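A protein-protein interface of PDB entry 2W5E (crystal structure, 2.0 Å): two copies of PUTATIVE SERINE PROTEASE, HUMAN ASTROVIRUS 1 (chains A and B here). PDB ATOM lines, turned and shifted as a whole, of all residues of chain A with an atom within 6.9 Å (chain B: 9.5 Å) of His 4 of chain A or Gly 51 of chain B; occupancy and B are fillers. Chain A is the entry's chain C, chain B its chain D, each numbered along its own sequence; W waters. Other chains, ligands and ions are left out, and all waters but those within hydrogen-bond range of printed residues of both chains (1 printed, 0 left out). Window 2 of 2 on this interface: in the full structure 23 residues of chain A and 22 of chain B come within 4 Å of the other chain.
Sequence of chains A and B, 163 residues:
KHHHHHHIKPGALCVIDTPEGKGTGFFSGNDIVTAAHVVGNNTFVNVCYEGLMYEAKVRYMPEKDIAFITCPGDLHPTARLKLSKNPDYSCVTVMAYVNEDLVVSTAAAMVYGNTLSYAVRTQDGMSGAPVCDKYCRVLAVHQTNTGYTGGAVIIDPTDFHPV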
ATOM      1  N   LYS A   1     -26.513 -26.237  33.716  1.00  0.00           N
ATOM      2  CA  LYS A   1     -27.614 -26.134  32.713  1.00  0.00           C
ATOM      3  C   LYS A   1     -28.563 -24.991  33.044  1.00  0.00           C
ATOM      4  O   LYS A   1     -29.035 -24.861  34.173  1.00  0.00           O
ATOM      5  CB  LYS A   1     -28.411 -27.438  32.630  1.00  0.00           C
ATOM      6  CG  LYS A   1     -27.828 -28.483  31.692  1.00  0.00           C
ATOM      7  CD  LYS A   1     -28.654 -29.765  31.736  1.00  0.00           C
ATOM      8  CE  LYS A   1     -28.092 -30.836  30.808  1.00  0.00           C
ATOM      9  NZ  LYS A   1     -28.934 -32.076  30.822  1.00  0.00           N
ATOM     10  N   HIS A   2     -28.839 -24.173  32.040  1.00  0.00           N
ATOM     11  CA  HIS A   2     -29.801 -23.090  32.160  1.00  0.00           C
ATOM     12  C   HIS A   2     -30.665 -23.076  30.916  1.00  0.00           C
ATOM     13  O   HIS A   2     -30.243 -23.536  29.852  1.00  0.00           O
ATOM     14  CB  HIS A   2     -29.084 -21.755  32.366  1.00  0.00           C
ATOM     15  CG  HIS A   2     -28.322 -21.689  33.650  1.00  0.00           C
ATOM     16  ND1 HIS A   2     -26.977 -21.979  33.736  1.00  0.00           N
ATOM     17  CD2 HIS A   2     -28.726 -21.412  34.911  1.00  0.00           C
ATOM     18  CE1 HIS A   2     -26.582 -21.864  34.990  1.00  0.00           C
ATOM     19  NE2 HIS A   2     -27.624 -21.522  35.724  1.00  0.00           N
ATOM     20  N   HIS A   3     -31.894 -22.595  31.064  1.00  0.00           N
ATOM     21  CA  HIS A   3     -32.779 -22.438  29.927  1.00  0.00           C
ATOM     22  C   HIS A   3     -32.471 -21.104  29.273  1.00  0.00           C
ATOM     23  O   HIS A   3     -32.919 -20.053  29.745  1.00  0.00           O
ATOM     24  CB  HIS A   3     -34.241 -22.498  30.361  1.00  0.00           C
ATOM     25  CG  HIS A   3     -34.677 -23.852  30.826  1.00  0.00           C
ATOM     26  ND1 HIS A   3     -34.944 -24.888  29.954  1.00  0.00           N
ATOM     27  CD2 HIS A   3     -34.899 -24.339  32.069  1.00  0.00           C
ATOM     28  CE1 HIS A   3     -35.302 -25.957  30.644  1.00  0.00           C
ATOM     29  NE2 HIS A   3     -35.287 -25.650  31.929  1.00  0.00           N
ATOM     30  N   HIS A   4     -31.689 -21.151  28.201  1.00  0.00           N
ATOM     31  CA  HIS A   4     -31.347 -19.952  27.445  1.00  0.00           C
ATOM     32  C   HIS A   4     -32.249 -19.852  26.214  1.00  0.00           C
ATOM     33  O   HIS A   4     -31.924 -20.355  25.146  1.00  0.00           O
ATOM     34  CB  HIS A   4     -29.846 -19.927  27.094  1.00  0.00           C
ATOM     35  CG  HIS A   4     -29.272 -21.274  26.762  1.00  0.00           C
ATOM     36  ND1 HIS A   4     -29.325 -21.815  25.495  1.00  0.00           N
ATOM     37  CD2 HIS A   4     -28.629 -22.186  27.531  1.00  0.00           C
ATOM     38  CE1 HIS A   4     -28.744 -23.004  25.497  1.00  0.00           C
ATOM     39  NE2 HIS A   4     -28.316 -23.254  26.722  1.00  0.00           N
ATOM     40  N   HIS A   5     -33.404 -19.213  26.389  1.00  0.00           N
ATOM     41  CA  HIS A   5     -34.448 -19.205  25.374  1.00  0.00           C
ATOM     42  C   HIS A   5     -34.367 -17.941  24.510  1.00  0.00           C
ATOM     43  O   HIS A   5     -33.630 -17.019  24.847  1.00  0.00           O
ATOM     44  CB  HIS A   5     -35.819 -19.351  26.037  1.00  0.00           C
ATOM     45  CG  HIS A   5     -36.087 -20.721  26.589  1.00  0.00           C
ATOM     46  ND1 HIS A   5     -37.352 -21.146  26.934  1.00  0.00           N
ATOM     47  CD2 HIS A   5     -35.260 -21.770  26.832  1.00  0.00           C
ATOM     48  CE1 HIS A   5     -37.293 -22.388  27.381  1.00  0.00           C
ATOM     49  NE2 HIS A   5     -36.036 -22.788  27.332  1.00  0.00           N
ATOM     50  N   HIS A   6     -35.103 -17.921  23.396  1.00  0.00           N
ATOM     51  CA  HIS A   6     -34.985 -16.846  22.386  1.00  0.00           C
ATOM     52  C   HIS A   6     -36.324 -16.317  21.867  1.00  0.00           C
ATOM     53  O   HIS A   6     -37.379 -16.891  22.142  1.00  0.00           O
ATOM     54  CB  HIS A   6     -34.127 -17.326  21.210  1.00  0.00           C
ATOM     55  CG  HIS A   6     -32.786 -17.828  21.633  1.00  0.00           C
ATOM     56  ND1 HIS A   6     -31.719 -16.988  21.856  1.00  0.00           N
ATOM     57  CD2 HIS A   6     -32.362 -19.073  21.945  1.00  0.00           C
ATOM     58  CE1 HIS A   6     -30.683 -17.699  22.266  1.00  0.00           C
ATOM     59  NE2 HIS A   6     -31.048 -18.968  22.326  1.00  0.00           N
ATOM     60  N   THR A 106     -39.015 -19.196  32.305  1.00  0.00           N
ATOM     61  CA  THR A 106     -38.778 -20.475  31.636  1.00  0.00           C
ATOM     62  C   THR A 106     -39.076 -21.634  32.591  1.00  0.00           C
ATOM     63  O   THR A 106     -39.135 -21.442  33.810  1.00  0.00           O
ATOM     64  CB  THR A 106     -37.327 -20.583  31.124  1.00  0.00           C
ATOM     65  OG1 THR A 106     -36.423 -20.405  32.218  1.00  0.00           O
ATOM     66  CG2 THR A 106     -37.042 -19.512  30.070  1.00  0.00           C
ATOM     67  N   LYS A 134     -38.682 -22.831  23.015  1.00  0.00           N
ATOM     68  CA  LYS A 134     -37.392 -22.170  23.219  1.00  0.00           C
ATOM     69  C   LYS A 134     -37.075 -21.099  22.173  1.00  0.00           C
ATOM     70  O   LYS A 134     -36.158 -20.304  22.362  1.00  0.00           O
ATOM     71  CB  LYS A 134     -36.259 -23.205  23.264  1.00  0.00           C
ATOM     72  CG  LYS A 134     -36.108 -24.040  21.987  1.00  0.00           C
ATOM     73  CD  LYS A 134     -35.537 -25.418  22.302  1.00  0.00           C
ATOM     74  CE  LYS A 134     -35.837 -26.415  21.185  1.00  0.00           C
ATOM     75  NZ  LYS A 134     -34.679 -26.689  20.287  1.00  0.00           N
ATOM     76  N   PRO B  10     -32.859 -11.160  26.845  1.00  0.00           N
ATOM     77  CA  PRO B  10     -32.402 -12.266  27.690  1.00  0.00           C
ATOM     78  C   PRO B  10     -31.106 -12.893  27.180  1.00  0.00           C
ATOM     79  O   PRO B  10     -30.360 -13.478  27.968  1.00  0.00           O
ATOM     80  CB  PRO B  10     -33.546 -13.278  27.585  1.00  0.00           C
ATOM     81  CG  PRO B  10     -34.734 -12.452  27.161  1.00  0.00           C
ATOM     82  CD  PRO B  10     -34.137 -11.494  26.197  1.00  0.00           C
ATOM     83  N   GLY B  11     -30.850 -12.759  25.877  1.00  0.00           N
ATOM     84  CA  GLY B  11     -29.581 -13.167  25.274  1.00  0.00           C
ATOM     85  C   GLY B  11     -28.394 -12.323  25.714  1.00  0.00           C
ATOM     86  O   GLY B  11     -27.247 -12.669  25.425  1.00  0.00           O
ATOM     87  N   ALA B  12     -28.660 -11.217  26.409  1.00  0.00           N
ATOM     88  CA  ALA B  12     -27.592 -10.399  26.981  1.00  0.00           C
ATOM     89  C   ALA B  12     -27.158 -10.880  28.378  1.00  0.00           C
ATOM     90  O   ALA B  12     -26.306 -10.262  29.016  1.00  0.00           O
ATOM     91  CB  ALA B  12     -27.997  -8.930  27.013  1.00  0.00           C
ATOM     92  N   LEU B  13     -27.748 -11.979  28.844  1.00  0.00           N
ATOM     93  CA  LEU B  13     -27.443 -12.517  30.167  1.00  0.00           C
ATOM     94  C   LEU B  13     -26.493 -13.710  30.098  1.00  0.00           C
ATOM     95  O   LEU B  13     -26.492 -14.455  29.118  1.00  0.00           O
ATOM     96  CB  LEU B  13     -28.727 -12.965  30.871  1.00  0.00           C
ATOM     97  CG  LEU B  13     -29.804 -11.951  31.258  1.00  0.00           C
ATOM     98  CD1 LEU B  13     -30.971 -12.688  31.886  1.00  0.00           C
ATOM     99  CD2 LEU B  13     -29.247 -10.914  32.211  1.00  0.00           C
ATOM    100  N   CYS B  14     -25.706 -13.889  31.157  1.00  0.00           N
ATOM    101  CA  CYS B  14     -24.914 -15.104  31.352  1.00  0.00           C
ATOM    102  C   CYS B  14     -24.918 -15.492  32.827  1.00  0.00           C
ATOM    103  O   CYS B  14     -25.525 -14.810  33.653  1.00  0.00           O
ATOM    104  CB  CYS B  14     -23.483 -14.922  30.840  1.00  0.00           C
ATOM    105  SG  CYS B  14     -22.543 -13.642  31.676  1.00  0.00           S
ATOM    106  N   VAL B  15     -24.251 -16.597  33.149  1.00  0.00           N
ATOM    107  CA  VAL B  15     -24.113 -17.044  34.531  1.00  0.00           C
ATOM    108  C   VAL B  15     -22.633 -17.051  34.923  1.00  0.00           C
ATOM    109  O   VAL B  15     -21.793 -17.575  34.190  1.00  0.00           O
ATOM    110  CB  VAL B  15     -24.751 -18.431  34.746  1.00  0.00           C
ATOM    111  CG1 VAL B  15     -24.523 -18.918  36.180  1.00  0.00           C
ATOM    112  CG2 VAL B  15     -26.252 -18.384  34.425  1.00  0.00           C
ATOM    113  N   VAL B  47     -17.573 -18.317  33.278  1.00  0.00           N
ATOM    114  CA  VAL B  47     -18.734 -17.711  32.630  1.00  0.00           C
ATOM    115  C   VAL B  47     -19.442 -18.783  31.817  1.00  0.00           C
ATOM    116  O   VAL B  47     -18.823 -19.448  30.981  1.00  0.00           O
ATOM    117  CB  VAL B  47     -18.327 -16.530  31.711  1.00  0.00           C
ATOM    118  CG1 VAL B  47     -19.528 -16.019  30.910  1.00  0.00           C
ATOM    119  CG2 VAL B  47     -17.708 -15.403  32.522  1.00  0.00           C
ATOM    120  N   CYS B  48     -20.731 -18.957  32.078  1.00  0.00           N
ATOM    121  CA  CYS B  48     -21.541 -19.925  31.352  1.00  0.00           C
ATOM    122  C   CYS B  48     -22.526 -19.230  30.410  1.00  0.00           C
ATOM    123  O   CYS B  48     -23.313 -18.382  30.845  1.00  0.00           O
ATOM    124  CB  CYS B  48     -22.280 -20.822  32.333  1.00  0.00           C
ATOM    125  SG  CYS B  48     -23.132 -22.157  31.529  1.00  0.00           S
ATOM    126  N   TYR B  49     -22.462 -19.579  29.124  1.00  0.00           N
ATOM    127  CA  TYR B  49     -23.295 -18.961  28.089  1.00  0.00           C
ATOM    128  C   TYR B  49     -23.648 -19.953  26.992  1.00  0.00           C
ATOM    129  O   TYR B  49     -22.760 -20.598  26.412  1.00  0.00           O
ATOM    130  CB  TYR B  49     -22.611 -17.721  27.487  1.00  0.00           C
ATOM    131  CG  TYR B  49     -23.491 -16.897  26.557  1.00  0.00           C
ATOM    132  CD1 TYR B  49     -24.476 -16.046  27.064  1.00  0.00           C
ATOM    133  CD2 TYR B  49     -23.331 -16.958  25.169  1.00  0.00           C
ATOM    134  CE1 TYR B  49     -25.286 -15.285  26.216  1.00  0.00           C
ATOM    135  CE2 TYR B  49     -24.135 -16.191  24.309  1.00  0.00           C
ATOM    136  CZ  TYR B  49     -25.110 -15.358  24.846  1.00  0.00           C
ATOM    137  OH  TYR B  49     -25.909 -14.602  24.017  1.00  0.00           O
ATOM    138  N   GLU B  50     -24.949 -20.070  26.720  1.00  0.00           N
ATOM    139  CA  GLU B  50     -25.492 -20.977  25.702  1.00  0.00           C
ATOM    140  C   GLU B  50     -24.923 -22.411  25.797  1.00  0.00           C
ATOM    141  O   GLU B  50     -24.756 -23.098  24.781  1.00  0.00           O
ATOM    142  CB  GLU B  50     -25.322 -20.380  24.293  1.00  0.00           C
ATOM    143  CG  GLU B  50     -26.363 -19.299  23.919  1.00  0.00           C
ATOM    144  CD  GLU B  50     -27.697 -19.880  23.488  1.00  0.00           C
ATOM    145  OE1 GLU B  50     -27.697 -20.768  22.614  1.00  0.00           O
ATOM    146  OE2 GLU B  50     -28.765 -19.467  24.011  1.00  0.00           O
ATOM    147  N   GLY B  51     -24.631 -22.847  27.023  1.00  0.00           N
ATOM    148  CA  GLY B  51     -24.147 -24.207  27.287  1.00  0.00           C
ATOM    149  C   GLY B  51     -22.637 -24.411  27.328  1.00  0.00           C
ATOM    150  O   GLY B  51     -22.166 -25.527  27.578  1.00  0.00           O
ATOM    151  N   LEU B  52     -21.876 -23.349  27.078  1.00  0.00           N
ATOM    152  CA  LEU B  52     -20.415 -23.423  27.095  1.00  0.00           C
ATOM    153  C   LEU B  52     -19.838 -22.582  28.228  1.00  0.00           C
ATOM    154  O   LEU B  52     -20.200 -21.410  28.393  1.00  0.00           O
ATOM    155  CB  LEU B  52     -19.823 -22.992  25.740  1.00  0.00           C
ATOM    156  CG  LEU B  52     -18.303 -23.094  25.506  1.00  0.00           C
ATOM    157  CD1 LEU B  52     -17.769 -24.506  25.767  1.00  0.00           C
ATOM    158  CD2 LEU B  52     -17.930 -22.635  24.096  1.00  0.00           C
ATOM    159  N   MET B  53     -18.956 -23.202  29.011  1.00  0.00           N
ATOM    160  CA  MET B  53     -18.255 -22.530  30.099  1.00  0.00           C
ATOM    161  C   MET B  53     -16.947 -21.938  29.588  1.00  0.00           C
ATOM    162  O   MET B  53     -16.217 -22.587  28.835  1.00  0.00           O
ATOM    163  CB  MET B  53     -17.951 -23.501  31.247  1.00  0.00           C
ATOM    164  CG  MET B  53     -19.145 -24.267  31.818  1.00  0.00           C
ATOM    165  SD  MET B  53     -20.012 -23.514  33.220  1.00  0.00           S
ATOM    166  CE  MET B  53     -18.680 -22.898  34.244  1.00  0.00           C
ATOM    167  N   TYR B  54     -16.660 -20.709  30.009  1.00  0.00           N
ATOM    168  CA  TYR B  54     -15.432 -20.006  29.645  1.00  0.00           C
ATOM    169  C   TYR B  54     -14.716 -19.573  30.912  1.00  0.00           C
ATOM    170  O   TYR B  54     -15.349 -19.387  31.953  1.00  0.00           O
ATOM    171  CB  TYR B  54     -15.739 -18.736  28.838  1.00  0.00           C
ATOM    172  CG  TYR B  54     -16.507 -18.916  27.544  1.00  0.00           C
ATOM    173  CD1 TYR B  54     -15.865 -18.798  26.310  1.00  0.00           C
ATOM    174  CD2 TYR B  54     -17.878 -19.162  27.548  1.00  0.00           C
ATOM    175  CE1 TYR B  54     -16.563 -18.939  25.117  1.00  0.00           C
ATOM    176  CE2 TYR B  54     -18.586 -19.309  26.357  1.00  0.00           C
ATOM    177  CZ  TYR B  54     -17.921 -19.192  25.150  1.00  0.00           C
ATOM    178  OH  TYR B  54     -18.619 -19.336  23.974  1.00  0.00           O
ATOM    179  N   LEU B  75     -16.223 -15.760  23.019  1.00  0.00           N
ATOM    180  CA  LEU B  75     -17.618 -15.672  23.450  1.00  0.00           C
ATOM    181  C   LEU B  75     -18.269 -14.484  22.732  1.00  0.00           C
ATOM    182  O   LEU B  75     -17.964 -13.329  23.023  1.00  0.00           O
ATOM    183  CB  LEU B  75     -17.693 -15.544  24.984  1.00  0.00           C
ATOM    184  CG  LEU B  75     -18.975 -15.146  25.734  1.00  0.00           C
ATOM    185  CD1 LEU B  75     -20.216 -15.798  25.171  1.00  0.00           C
ATOM    186  CD2 LEU B  75     -18.840 -15.464  27.212  1.00  0.00           C
ATOM    187  N   THR B  78     -25.116 -12.794  21.638  1.00  0.00           N
ATOM    188  CA  THR B  78     -26.128 -12.369  20.664  1.00  0.00           C
ATOM    189  C   THR B  78     -26.752 -11.005  20.999  1.00  0.00           C
ATOM    190  O   THR B  78     -27.350 -10.360  20.130  1.00  0.00           O
ATOM    191  CB  THR B  78     -27.243 -13.418  20.490  1.00  0.00           C
ATOM    192  OG1 THR B  78     -27.994 -13.531  21.704  1.00  0.00           O
ATOM    193  CG2 THR B  78     -26.653 -14.785  20.121  1.00  0.00           C
ATOM    194  N   TYR B  97     -31.150 -14.932  35.908  1.00  0.00           N
ATOM    195  CA  TYR B  97     -31.165 -16.387  36.037  1.00  0.00           C
ATOM    196  C   TYR B  97     -31.342 -16.760  37.505  1.00  0.00           C
ATOM    197  O   TYR B  97     -30.586 -16.318  38.365  1.00  0.00           O
ATOM    198  CB  TYR B  97     -29.898 -17.040  35.452  1.00  0.00           C
ATOM    199  CG  TYR B  97     -29.919 -17.160  33.946  1.00  0.00           C
ATOM    200  CD1 TYR B  97     -30.855 -17.975  33.309  1.00  0.00           C
ATOM    201  CD2 TYR B  97     -29.010 -16.455  33.158  1.00  0.00           C
ATOM    202  CE1 TYR B  97     -30.888 -18.087  31.927  1.00  0.00           C
ATOM    203  CE2 TYR B  97     -29.028 -16.567  31.767  1.00  0.00           C
ATOM    204  CZ  TYR B  97     -29.977 -17.381  31.163  1.00  0.00           C
ATOM    205  OH  TYR B  97     -30.020 -17.494  29.795  1.00  0.00           O
ATOM    206  N   ASN B  99     -31.571 -20.179  39.544  1.00  0.00           N
ATOM    207  CA  ASN B  99     -31.294 -21.604  39.336  1.00  0.00           C
ATOM    208  C   ASN B  99     -31.191 -21.884  37.832  1.00  0.00           C
ATOM    209  O   ASN B  99     -30.389 -21.248  37.153  1.00  0.00           O
ATOM    210  CB  ASN B  99     -32.342 -22.488  40.042  1.00  0.00           C
ATOM    211  CG  ASN B  99     -32.389 -22.251  41.551  1.00  0.00           C
ATOM    212  OD1 ASN B  99     -31.361 -22.018  42.193  1.00  0.00           O
ATOM    213  ND2 ASN B  99     -33.588 -22.314  42.122  1.00  0.00           N
ATOM    214  N   GLU B 100     -32.011 -22.791  37.308  1.00  0.00           N
ATOM    215  CA  GLU B 100     -31.982 -23.122  35.875  1.00  0.00           C
ATOM    216  C   GLU B 100     -32.773 -22.148  34.995  1.00  0.00           C
ATOM    217  O   GLU B 100     -32.667 -22.190  33.767  1.00  0.00           O
ATOM    218  CB  GLU B 100     -32.496 -24.549  35.639  1.00  0.00           C
ATOM    219  CG  GLU B 100     -31.556 -25.635  36.159  1.00  0.00           C
ATOM    220  CD  GLU B 100     -32.128 -27.040  36.043  1.00  0.00           C
ATOM    221  OE1 GLU B 100     -33.128 -27.237  35.308  1.00  0.00           O
ATOM    222  OE2 GLU B 100     -31.567 -27.955  36.693  1.00  0.00           O
ATOM    223  N   ASP B 101     -33.556 -21.272  35.620  1.00  0.00           N
ATOM    224  CA  ASP B 101     -34.593 -20.540  34.896  1.00  0.00           C
ATOM    225  C   ASP B 101     -34.321 -19.052  34.699  1.00  0.00           C
ATOM    226  O   ASP B 101     -33.803 -18.374  35.585  1.00  0.00           O
ATOM    227  CB  ASP B 101     -35.950 -20.707  35.588  1.00  0.00           C
ATOM    228  CG  ASP B 101     -36.385 -22.159  35.696  1.00  0.00           C
ATOM    229  OD1 ASP B 101     -36.449 -22.860  34.660  1.00  0.00           O
ATOM    230  OD2 ASP B 101     -36.687 -22.590  36.828  1.00  0.00           O
ATOM    231  N   LEU B 102     -34.698 -18.558  33.521  1.00  0.00           N
ATOM    232  CA  LEU B 102     -34.790 -17.132  33.285  1.00  0.00           C
ATOM    233  C   LEU B 102     -36.023 -16.601  34.016  1.00  0.00           C
ATOM    234  O   LEU B 102     -37.092 -17.207  33.967  1.00  0.00           O
ATOM    235  CB  LEU B 102     -34.913 -16.831  31.783  1.00  0.00           C
ATOM    236  CG  LEU B 102     -35.257 -15.375  31.411  1.00  0.00           C
ATOM    237  CD1 LEU B 102     -34.078 -14.468  31.680  1.00  0.00           C
ATOM    238  CD2 LEU B 102     -35.723 -15.239  29.964  1.00  0.00           C
HETATM  239  O   HOH W   1     -26.405 -23.615  29.839  1.00  0.00           O
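A ring nitrogen (NE2) of His 2 of chain A lies close to the backbone carbonyl oxygen (O) of Asn 99 of chain B, 3.1 Å away.
The backbone carbonyl oxygen of Glu 100 of chain B sits at hydrogen-bond distance from the backbone NH of His 3 of chain A (2.8 Å).
The side-chain carboxylate (OD1) of Asp 101 of chain B sits close to the side-chain hydroxyl (OG1) of Thr 106 of chain A (3.5 Å).
OG1 of Thr 106 of chain A is in hydrogen-bond range of N of Leu 102 of chain B (2.8 Å).
ND1 of His 4 of chain A sits close to OE2 of Glu 50 of chain B.
A ring nitrogen (NE2) of His 6 of chain A sits close to the side-chain carboxylate (OE2) of Glu 50 of chain B, 2.9 Å away.
N of His 6 of chain A is in hydrogen-bond range of O of Lys 134 of chain A (2.8 Å).
The backbone NH (N) of Cys 48 of chain B is in hydrogen-bond range of the backbone carbonyl oxygen (O) of Val 15 of chain B, at 2.7 Å.
Glu 100 of chain B touches Lys 1 of chain A (CG to O, 3.3 Å).
Val 15 of chain B touches His 2 of chain A (CG2 to CE1, 3.5 Å).
Glu 100 of chain B touches His 2 of chain A.
Tyr 97 of chain B touches His 3 of chain A.
His 3 of chain A touches Asp 101 of chain B (CD2 to OD1, 3.4 Å).
His 4 of chain A touches Gly 51 of chain B.
Tyr 97 of chain B touches His 4 of chain A (OH to CB, 3.6 Å).
His 4 of chain A touches three residues of chain B.
Of the printed residues of chain B, His 6 of chain A touches Glu 50.
Cys 48 of chain B touches none of the printed residues of chain A.
Gly 51 of chain B touches just one residue of chain A: His 4 (3.7 Å).
Printed residues of chain A within 4 Å of Asn 99 of chain B: His 2.
The nearest residue of chain B that does not touch His 4 of chain A is Tyr 49 of chain B (5.5 Å).
Of the 21 printed residues of chain B, 8 touch a printed residue of chain A.
Hydrophobic or aromatic side chains of chain B within 4 Å of the printed part of chain A: Val 15, Tyr 97 and Leu 102.
Along chain A the printed residues that touch a printed residue of chain B span positions 1 to 106.
No position is printed for both chains.
Of the 13 pairs that touch across the chains among the printed residues, none has its exchanged pair printed and touching as well.
Water W1 bridges N of His 2 of chain A and N of Gly 51 of chain B.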
